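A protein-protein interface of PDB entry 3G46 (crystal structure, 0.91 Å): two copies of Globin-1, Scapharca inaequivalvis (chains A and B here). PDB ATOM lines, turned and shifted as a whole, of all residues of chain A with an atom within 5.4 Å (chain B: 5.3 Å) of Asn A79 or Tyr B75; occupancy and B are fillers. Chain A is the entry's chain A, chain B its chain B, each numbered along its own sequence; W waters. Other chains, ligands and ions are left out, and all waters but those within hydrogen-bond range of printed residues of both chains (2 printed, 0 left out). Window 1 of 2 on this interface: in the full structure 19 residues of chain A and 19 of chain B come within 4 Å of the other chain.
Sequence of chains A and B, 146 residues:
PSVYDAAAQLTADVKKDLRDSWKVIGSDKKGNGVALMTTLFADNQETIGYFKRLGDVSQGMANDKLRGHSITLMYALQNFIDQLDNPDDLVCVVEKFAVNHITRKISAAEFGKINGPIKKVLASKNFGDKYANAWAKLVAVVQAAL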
ATOM      1  N   MET A  74      22.470  20.897  23.463  1.00  0.00           N
ATOM      2  CA  MET A  74      21.144  21.474  23.225  1.00  0.00           C
ATOM      3  C   MET A  74      20.688  21.285  21.786  1.00  0.00           C
ATOM      4  O   MET A  74      19.468  21.236  21.537  1.00  0.00           O
ATOM      5  CB  MET A  74      21.170  22.957  23.622  1.00  0.00           C
ATOM      6  CG  MET A  74      21.446  23.158  25.106  1.00  0.00           C
ATOM      7  SD  MET A  74      20.138  22.528  26.163  1.00  0.00           S
ATOM      8  CE  MET A  74      18.996  23.908  26.064  1.00  0.00           C
ATOM      9  N   TYR A  75      21.598  21.165  20.828  1.00  0.00           N
ATOM     10  CA  TYR A  75      21.212  20.823  19.457  1.00  0.00           C
ATOM     11  C   TYR A  75      20.863  19.350  19.318  1.00  0.00           C
ATOM     12  O   TYR A  75      20.098  19.016  18.406  1.00  0.00           O
ATOM     13  CB  TYR A  75      22.322  21.215  18.420  1.00  0.00           C
ATOM     14  CG  TYR A  75      22.232  22.720  18.224  1.00  0.00           C
ATOM     15  CD1 TYR A  75      21.324  23.284  17.333  1.00  0.00           C
ATOM     16  CD2 TYR A  75      23.061  23.558  18.952  1.00  0.00           C
ATOM     17  CE1 TYR A  75      21.252  24.657  17.170  1.00  0.00           C
ATOM     18  CE2 TYR A  75      22.994  24.925  18.799  1.00  0.00           C
ATOM     19  CZ  TYR A  75      22.094  25.460  17.909  1.00  0.00           C
ATOM     20  OH  TYR A  75      22.086  26.817  17.818  1.00  0.00           O
ATOM     21  N   ALA A  76      21.370  18.469  20.175  1.00  0.00           N
ATOM     22  CA  ALA A  76      20.830  17.109  20.209  1.00  0.00           C
ATOM     23  C   ALA A  76      19.363  17.131  20.627  1.00  0.00           C
ATOM     24  O   ALA A  76      18.516  16.460  20.043  1.00  0.00           O
ATOM     25  CB  ALA A  76      21.658  16.234  21.132  1.00  0.00           C
ATOM     26  N   LEU A  77      19.062  17.925  21.659  1.00  0.00           N
ATOM     27  CA  LEU A  77      17.654  18.054  22.076  1.00  0.00           C
ATOM     28  C   LEU A  77      16.799  18.678  20.978  1.00  0.00           C
ATOM     29  O   LEU A  77      15.676  18.219  20.738  1.00  0.00           O
ATOM     30  CB  LEU A  77      17.576  18.861  23.374  1.00  0.00           C
ATOM     31  CG  LEU A  77      18.285  18.229  24.567  1.00  0.00           C
ATOM     32  CD1 LEU A  77      18.027  19.051  25.822  1.00  0.00           C
ATOM     33  CD2 LEU A  77      17.849  16.787  24.791  1.00  0.00           C
ATOM     34  N   GLN A  78      17.302  19.706  20.302  1.00  0.00           N
ATOM     35  CA  GLN A  78      16.577  20.306  19.188  1.00  0.00           C
ATOM     36  C   GLN A  78      16.231  19.279  18.118  1.00  0.00           C
ATOM     37  O   GLN A  78      15.122  19.222  17.583  1.00  0.00           O
ATOM     38  CB  GLN A  78      17.412  21.444  18.586  1.00  0.00           C
ATOM     39  CG  GLN A  78      16.711  22.155  17.442  1.00  0.00           C
ATOM     40  CD  GLN A  78      15.626  23.055  17.950  1.00  0.00           C
ATOM     41  OE1 GLN A  78      15.881  23.923  18.791  1.00  0.00           O
ATOM     42  NE2 GLN A  78      14.438  22.816  17.430  1.00  0.00           N
ATOM     43  N   ASN A  79      17.228  18.450  17.804  1.00  0.00           N
ATOM     44  CA  ASN A  79      17.085  17.360  16.842  1.00  0.00           C
ATOM     45  C   ASN A  79      15.952  16.446  17.285  1.00  0.00           C
ATOM     46  O   ASN A  79      15.024  16.148  16.512  1.00  0.00           O
ATOM     47  CB  ASN A  79      18.466  16.721  16.741  1.00  0.00           C
ATOM     48  CG  ASN A  79      18.680  15.614  15.767  1.00  0.00           C
ATOM     49  OD1 ASN A  79      19.848  15.183  15.553  1.00  0.00           O
ATOM     50  ND2 ASN A  79      17.621  15.139  15.171  1.00  0.00           N
ATOM     51  N   PHE A  80      15.986  15.979  18.540  1.00  0.00           N
ATOM     52  CA  PHE A  80      14.901  15.113  18.999  1.00  0.00           C
ATOM     53  C   PHE A  80      13.522  15.755  18.862  1.00  0.00           C
ATOM     54  O   PHE A  80      12.573  15.125  18.378  1.00  0.00           O
ATOM     55  CB  PHE A  80      15.105  14.725  20.462  1.00  0.00           C
ATOM     56  CG  PHE A  80      16.347  13.907  20.762  1.00  0.00           C
ATOM     57  CD1 PHE A  80      16.961  13.129  19.805  1.00  0.00           C
ATOM     58  CD2 PHE A  80      16.891  13.930  22.032  1.00  0.00           C
ATOM     59  CE1 PHE A  80      18.090  12.402  20.126  1.00  0.00           C
ATOM     60  CE2 PHE A  80      18.021  13.209  22.360  1.00  0.00           C
ATOM     61  CZ  PHE A  80      18.625  12.436  21.392  1.00  0.00           C
ATOM     62  N   ILE A  81      13.399  17.006  19.288  1.00  0.00           N
ATOM     63  CA  ILE A  81      12.120  17.710  19.178  1.00  0.00           C
ATOM     64  C   ILE A  81      11.658  17.755  17.729  1.00  0.00           C
ATOM     65  O   ILE A  81      10.487  17.533  17.426  1.00  0.00           O
ATOM     66  CB  ILE A  81      12.246  19.119  19.786  1.00  0.00           C
ATOM     67  CG1 ILE A  81      12.525  19.077  21.294  1.00  0.00           C
ATOM     68  CG2 ILE A  81      11.031  19.978  19.479  1.00  0.00           C
ATOM     69  CD1 ILE A  81      11.379  18.488  22.104  1.00  0.00           C
ATOM     70  N   ASP A  82      12.572  18.042  16.810  1.00  0.00           N
ATOM     71  CA  ASP A  82      12.203  18.145  15.405  1.00  0.00           C
ATOM     72  C   ASP A  82      11.828  16.789  14.805  1.00  0.00           C
ATOM     73  O   ASP A  82      11.145  16.793  13.777  1.00  0.00           O
ATOM     74  CB  ASP A  82      13.361  18.779  14.638  1.00  0.00           C
ATOM     75  CG  ASP A  82      13.556  20.264  14.857  1.00  0.00           C
ATOM     76  OD1 ASP A  82      12.634  20.927  15.384  1.00  0.00           O
ATOM     77  OD2 ASP A  82      14.648  20.770  14.496  1.00  0.00           O
ATOM     78  N   GLN A  83      12.232  15.668  15.398  1.00  0.00           N
ATOM     79  CA  GLN A  83      11.889  14.350  14.880  1.00  0.00           C
ATOM     80  C   GLN A  83      10.670  13.717  15.549  1.00  0.00           C
ATOM     81  O   GLN A  83      10.337  12.564  15.267  1.00  0.00           O
ATOM     82  CB  GLN A  83      13.033  13.343  15.053  1.00  0.00           C
ATOM     83  CG  GLN A  83      14.394  13.742  14.564  1.00  0.00           C
ATOM     84  CD  GLN A  83      14.400  14.624  13.327  1.00  0.00           C
ATOM     85  OE1 GLN A  83      15.144  15.621  13.316  1.00  0.00           O
ATOM     86  NE2 GLN A  83      13.599  14.262  12.335  1.00  0.00           N
ATOM     87  N   LEU A  84       9.973  14.410  16.437  1.00  0.00           N
ATOM     88  CA  LEU A  84       8.903  13.744  17.183  1.00  0.00           C
ATOM     89  C   LEU A  84       7.782  13.215  16.289  1.00  0.00           C
ATOM     90  O   LEU A  84       7.094  12.272  16.710  1.00  0.00           O
ATOM     91  CB  LEU A  84       8.299  14.695  18.220  1.00  0.00           C
ATOM     92  CG  LEU A  84       9.179  15.163  19.368  1.00  0.00           C
ATOM     93  CD1 LEU A  84       8.508  16.296  20.134  1.00  0.00           C
ATOM     94  CD2 LEU A  84       9.507  14.032  20.335  1.00  0.00           C
ATOM     95  N   VAL A  93      18.047   8.937  15.243  1.00  0.00           N
ATOM     96  CA  VAL A  93      18.950   9.946  15.855  1.00  0.00           C
ATOM     97  C   VAL A  93      19.192   9.585  17.314  1.00  0.00           C
ATOM     98  O   VAL A  93      20.324   9.780  17.788  1.00  0.00           O
ATOM     99  CB  VAL A  93      18.440  11.389  15.691  1.00  0.00           C
ATOM    100  CG1 VAL A  93      18.388  11.635  14.185  1.00  0.00           C
ATOM    101  CG2 VAL A  93      17.103  11.694  16.321  1.00  0.00           C
ATOM    102  N   PHE A  97      23.029   9.008  19.082  1.00  0.00           N
ATOM    103  CA  PHE A  97      23.565   9.555  20.333  1.00  0.00           C
ATOM    104  C   PHE A  97      23.769   8.466  21.375  1.00  0.00           C
ATOM    105  O   PHE A  97      24.664   8.601  22.219  1.00  0.00           O
ATOM    106  CB  PHE A  97      22.662  10.671  20.894  1.00  0.00           C
ATOM    107  CG  PHE A  97      22.717  11.914  20.026  1.00  0.00           C
ATOM    108  CD1 PHE A  97      23.870  12.660  19.907  1.00  0.00           C
ATOM    109  CD2 PHE A  97      21.583  12.303  19.326  1.00  0.00           C
ATOM    110  CE1 PHE A  97      23.881  13.782  19.095  1.00  0.00           C
ATOM    111  CE2 PHE A  97      21.587  13.423  18.525  1.00  0.00           C
ATOM    112  CZ  PHE A  97      22.747  14.166  18.408  1.00  0.00           C
ATOM    113  N   LYS B  29      16.480  18.813   6.594  1.00  0.00           N
ATOM    114  CA  LYS B  29      17.747  18.288   7.097  1.00  0.00           C
ATOM    115  C   LYS B  29      17.924  16.836   6.688  1.00  0.00           C
ATOM    116  O   LYS B  29      19.025  16.439   6.294  1.00  0.00           O
ATOM    117  CB  LYS B  29      17.821  18.462   8.614  1.00  0.00           C
ATOM    118  CG  LYS B  29      17.995  19.922   9.009  1.00  0.00           C
ATOM    119  CD  LYS B  29      18.180  20.075  10.502  1.00  0.00           C
ATOM    120  CE  LYS B  29      18.538  21.477  10.932  1.00  0.00           C
ATOM    121  NZ  LYS B  29      17.485  22.472  10.620  1.00  0.00           N
ATOM    122  N   ILE B  71      21.203  13.485   9.467  1.00  0.00           N
ATOM    123  CA  ILE B  71      20.390  14.494  10.165  1.00  0.00           C
ATOM    124  C   ILE B  71      21.238  15.212  11.203  1.00  0.00           C
ATOM    125  O   ILE B  71      21.218  16.439  11.325  1.00  0.00           O
ATOM    126  CB  ILE B  71      19.144  13.836  10.782  1.00  0.00           C
ATOM    127  CG1 ILE B  71      18.186  13.288   9.727  1.00  0.00           C
ATOM    128  CG2 ILE B  71      18.419  14.787  11.732  1.00  0.00           C
ATOM    129  CD1 ILE B  71      17.115  12.358  10.252  1.00  0.00           C
ATOM    130  N   THR B  72      22.015  14.445  11.981  1.00  0.00           N
ATOM    131  CA  THR B  72      22.800  15.047  13.063  1.00  0.00           C
ATOM    132  C   THR B  72      23.877  15.968  12.498  1.00  0.00           C
ATOM    133  O   THR B  72      24.157  17.020  13.088  1.00  0.00           O
ATOM    134  CB  THR B  72      23.365  13.924  13.958  1.00  0.00           C
ATOM    135  OG1 THR B  72      22.238  13.197  14.496  1.00  0.00           O
ATOM    136  CG2 THR B  72      24.198  14.503  15.093  1.00  0.00           C
ATOM    137  N   LEU B  73      24.487  15.612  11.373  1.00  0.00           N
ATOM    138  CA  LEU B  73      25.453  16.498  10.726  1.00  0.00           C
ATOM    139  C   LEU B  73      24.800  17.840  10.408  1.00  0.00           C
ATOM    140  O   LEU B  73      25.426  18.901  10.560  1.00  0.00           O
ATOM    141  CB  LEU B  73      26.020  15.829   9.473  1.00  0.00           C
ATOM    142  CG  LEU B  73      27.017  16.647   8.656  1.00  0.00           C
ATOM    143  CD1 LEU B  73      28.034  15.696   8.022  1.00  0.00           C
ATOM    144  CD2 LEU B  73      26.361  17.509   7.585  1.00  0.00           C
ATOM    145  N   MET B  74      23.553  17.811   9.955  1.00  0.00           N
ATOM    146  CA  MET B  74      22.874  19.062   9.623  1.00  0.00           C
ATOM    147  C   MET B  74      22.616  19.908  10.865  1.00  0.00           C
ATOM    148  O   MET B  74      22.538  21.138  10.745  1.00  0.00           O
ATOM    149  CB  MET B  74      21.571  18.750   8.870  1.00  0.00           C
ATOM    150  CG  MET B  74      21.818  18.060   7.541  1.00  0.00           C
ATOM    151  SD  MET B  74      22.626  19.090   6.316  1.00  0.00           S
ATOM    152  CE  MET B  74      21.243  20.000   5.642  1.00  0.00           C
ATOM    153  N   TYR B  75      22.484  19.289  12.044  1.00  0.00           N
ATOM    154  CA  TYR B  75      22.389  20.087  13.271  1.00  0.00           C
ATOM    155  C   TYR B  75      23.744  20.641  13.689  1.00  0.00           C
ATOM    156  O   TYR B  75      23.764  21.658  14.394  1.00  0.00           O
ATOM    157  CB  TYR B  75      21.757  19.292  14.453  1.00  0.00           C
ATOM    158  CG  TYR B  75      20.256  19.230  14.217  1.00  0.00           C
ATOM    159  CD1 TYR B  75      19.427  20.267  14.613  1.00  0.00           C
ATOM    160  CD2 TYR B  75      19.690  18.133  13.583  1.00  0.00           C
ATOM    161  CE1 TYR B  75      18.055  20.194  14.384  1.00  0.00           C
ATOM    162  CE2 TYR B  75      18.342  18.054  13.349  1.00  0.00           C
ATOM    163  CZ  TYR B  75      17.531  19.092  13.756  1.00  0.00           C
ATOM    164  OH  TYR B  75      16.190  18.951  13.489  1.00  0.00           O
ATOM    165  N   ALA B  76      24.859  20.042  13.304  1.00  0.00           N
ATOM    166  CA  ALA B  76      26.158  20.683  13.497  1.00  0.00           C
ATOM    167  C   ALA B  76      26.199  21.979  12.693  1.00  0.00           C
ATOM    168  O   ALA B  76      26.629  23.035  13.167  1.00  0.00           O
ATOM    169  CB  ALA B  76      27.299  19.746  13.128  1.00  0.00           C
ATOM    170  N   LEU B  77      25.743  21.910  11.435  1.00  0.00           N
ATOM    171  CA  LEU B  77      25.700  23.112  10.600  1.00  0.00           C
ATOM    172  C   LEU B  77      24.730  24.142  11.175  1.00  0.00           C
ATOM    173  O   LEU B  77      25.050  25.328  11.193  1.00  0.00           O
ATOM    174  CB  LEU B  77      25.329  22.738   9.167  1.00  0.00           C
ATOM    175  CG  LEU B  77      26.318  21.812   8.462  1.00  0.00           C
ATOM    176  CD1 LEU B  77      25.900  21.595   7.023  1.00  0.00           C
ATOM    177  CD2 LEU B  77      27.735  22.376   8.521  1.00  0.00           C
ATOM    178  N   GLN B  78      23.559  23.717  11.648  1.00  0.00           N
ATOM    179  CA  GLN B  78      22.629  24.647  12.283  1.00  0.00           C
ATOM    180  C   GLN B  78      23.280  25.402  13.433  1.00  0.00           C
ATOM    181  O   GLN B  78      23.116  26.619  13.576  1.00  0.00           O
ATOM    182  CB  GLN B  78      21.392  23.898  12.799  1.00  0.00           C
ATOM    183  CG  GLN B  78      20.360  24.819  13.428  1.00  0.00           C
ATOM    184  CD  GLN B  78      19.588  25.582  12.377  1.00  0.00           C
ATOM    185  OE1 GLN B  78      19.052  24.961  11.457  1.00  0.00           O
ATOM    186  NE2 GLN B  78      19.539  26.901  12.510  1.00  0.00           N
ATOM    187  N   ASN B  79      24.006  24.655  14.248  1.00  0.00           N
ATOM    188  CA  ASN B  79      24.750  25.197  15.391  1.00  0.00           C
ATOM    189  C   ASN B  79      25.719  26.248  14.900  1.00  0.00           C
ATOM    190  O   ASN B  79      25.730  27.378  15.396  1.00  0.00           O
ATOM    191  CB  ASN B  79      25.361  23.988  16.096  1.00  0.00           C
ATOM    192  CG  ASN B  79      26.122  24.295  17.362  1.00  0.00           C
ATOM    193  OD1 ASN B  79      26.361  25.436  17.738  1.00  0.00           O
ATOM    194  ND2 ASN B  79      26.514  23.198  18.019  1.00  0.00           N
ATOM    195  N   PHE B  80      26.552  25.927  13.913  1.00  0.00           N
ATOM    196  CA  PHE B  80      27.480  26.924  13.394  1.00  0.00           C
ATOM    197  C   PHE B  80      26.772  28.186  12.916  1.00  0.00           C
ATOM    198  O   PHE B  80      27.193  29.303  13.234  1.00  0.00           O
ATOM    199  CB  PHE B  80      28.296  26.358  12.227  1.00  0.00           C
ATOM    200  CG  PHE B  80      29.205  25.195  12.527  1.00  0.00           C
ATOM    201  CD1 PHE B  80      29.678  24.936  13.798  1.00  0.00           C
ATOM    202  CD2 PHE B  80      29.583  24.351  11.499  1.00  0.00           C
ATOM    203  CE1 PHE B  80      30.514  23.860  14.024  1.00  0.00           C
ATOM    204  CE2 PHE B  80      30.414  23.267  11.716  1.00  0.00           C
ATOM    205  CZ  PHE B  80      30.874  23.024  12.990  1.00  0.00           C
HETATM  206  O   HOH W   1      14.924  21.290  11.397  1.00  0.00           O
HETATM  207  O   HOH W   2      14.635  17.937  11.067  1.00  0.00           O
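The side-chain amide oxygen of Asn A79 lies within hydrogen-bond range of the side-chain hydroxyl of Thr B72 (3.3 Å). OD2 of Asp A82 is in hydrogen-bond range of OH of Tyr B75 (2.6 Å). The side-chain hydroxyl (OH) of Tyr B75 is in hydrogen-bond range of the side-chain amide oxygen (OE1) of Gln A83 (3.5 Å).
Water W1 lies within hydrogen-bond range of NZ of Lys B29 (2.9 Å), OD2 of Asp A82 (3.2 Å) and OH of Tyr B75 (3.4 Å). Water W2 lies within hydrogen-bond range of the side-chain hydroxyl (OH) of Tyr B75 (3.1 Å) and the side-chain amide oxygen (OE1) of Gln A83 (3.3 Å).
Among the printed residues, merely in contact across the chains: Tyr A75 with Gln B78 (3.9 Å), Tyr A75 with Asn B79 (3.5 Å), Gln A78 with Tyr B75 (3.9 Å), Asn A79 with Ile B71 (3.5 Å), Asn A79 with Tyr B75 (3.5 Å), Gln A83 with Ile B71 (3.7 Å), Val A93 with Ile B71 (3.99 Å) and Phe A97 with Thr B72 (3.6 Å).
ND2 of Asn A79 is in hydrogen-bond range of OE1 of Gln A83. OD1 of Asp A82 sits at hydrogen-bond distance from NE2 of Gln A78. The side-chain amino group of Lys B29 lies within hydrogen-bond range of the side-chain amide oxygen of Gln B78 (3.1 Å).
Printed residues of chain A that touch a printed residue of chain B: Tyr A75, Gln A78, Asn A79, Asp A82, Gln A83, Val A93 and Phe A97. Of the 11 printed residues of chain B, 5 touch a printed residue of chain A. Printed residues of chain B that touch a printed residue of chain A: Ile B71, Thr B72, Tyr B75, Gln B78 and Asn B79. Hydrophobic or aromatic side chains of chain B that line the printed part of chain A: Ile B71 and Tyr B75. Among the printed residues, no Asp or Glu carboxylate lies within 4 Å of a Lys or Arg side-chain nitrogen of the other chain.
Asn A79 touches just these residues of chain B: Ile B71, Thr B72 and Tyr B75. Of chain A, only Gln A78, Asn A79, Asp A82 and Gln A83 come within 4 Å of Tyr B75. Printed residues of chain B within 4 Å of Asp A82: Tyr B75. Of the printed residues of chain B, Gln A78 touches Tyr B75. Printed residues of chain A within 4 Å of Gln B78: Tyr A75 (3.9 Å). Of the printed residues of chain A, Ile B71 touches Asn A79 (3.5 Å), Gln A83 (3.7 Å) and Val A93 (3.99 Å). The nearest printed residue of chain B that does not touch Asn A79 is Leu B73 (6.3 Å). The nearest printed residue of chain B that does not touch Gln A83 is Lys B29 (6.1 Å).
Tyr A75 touches Gln B78, and with the chains exchanged Gln A78 touches Tyr B75. Tyr A75 touches Asn B79, and with the chains exchanged Asn A79 touches Tyr B75. Positions printed for both chains: 74, 75, 76, 77, 78, 79 and 80. Of the 11 pairs that touch across the chains among the printed residues, 4 have their exchanged pair printed and touching as well.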
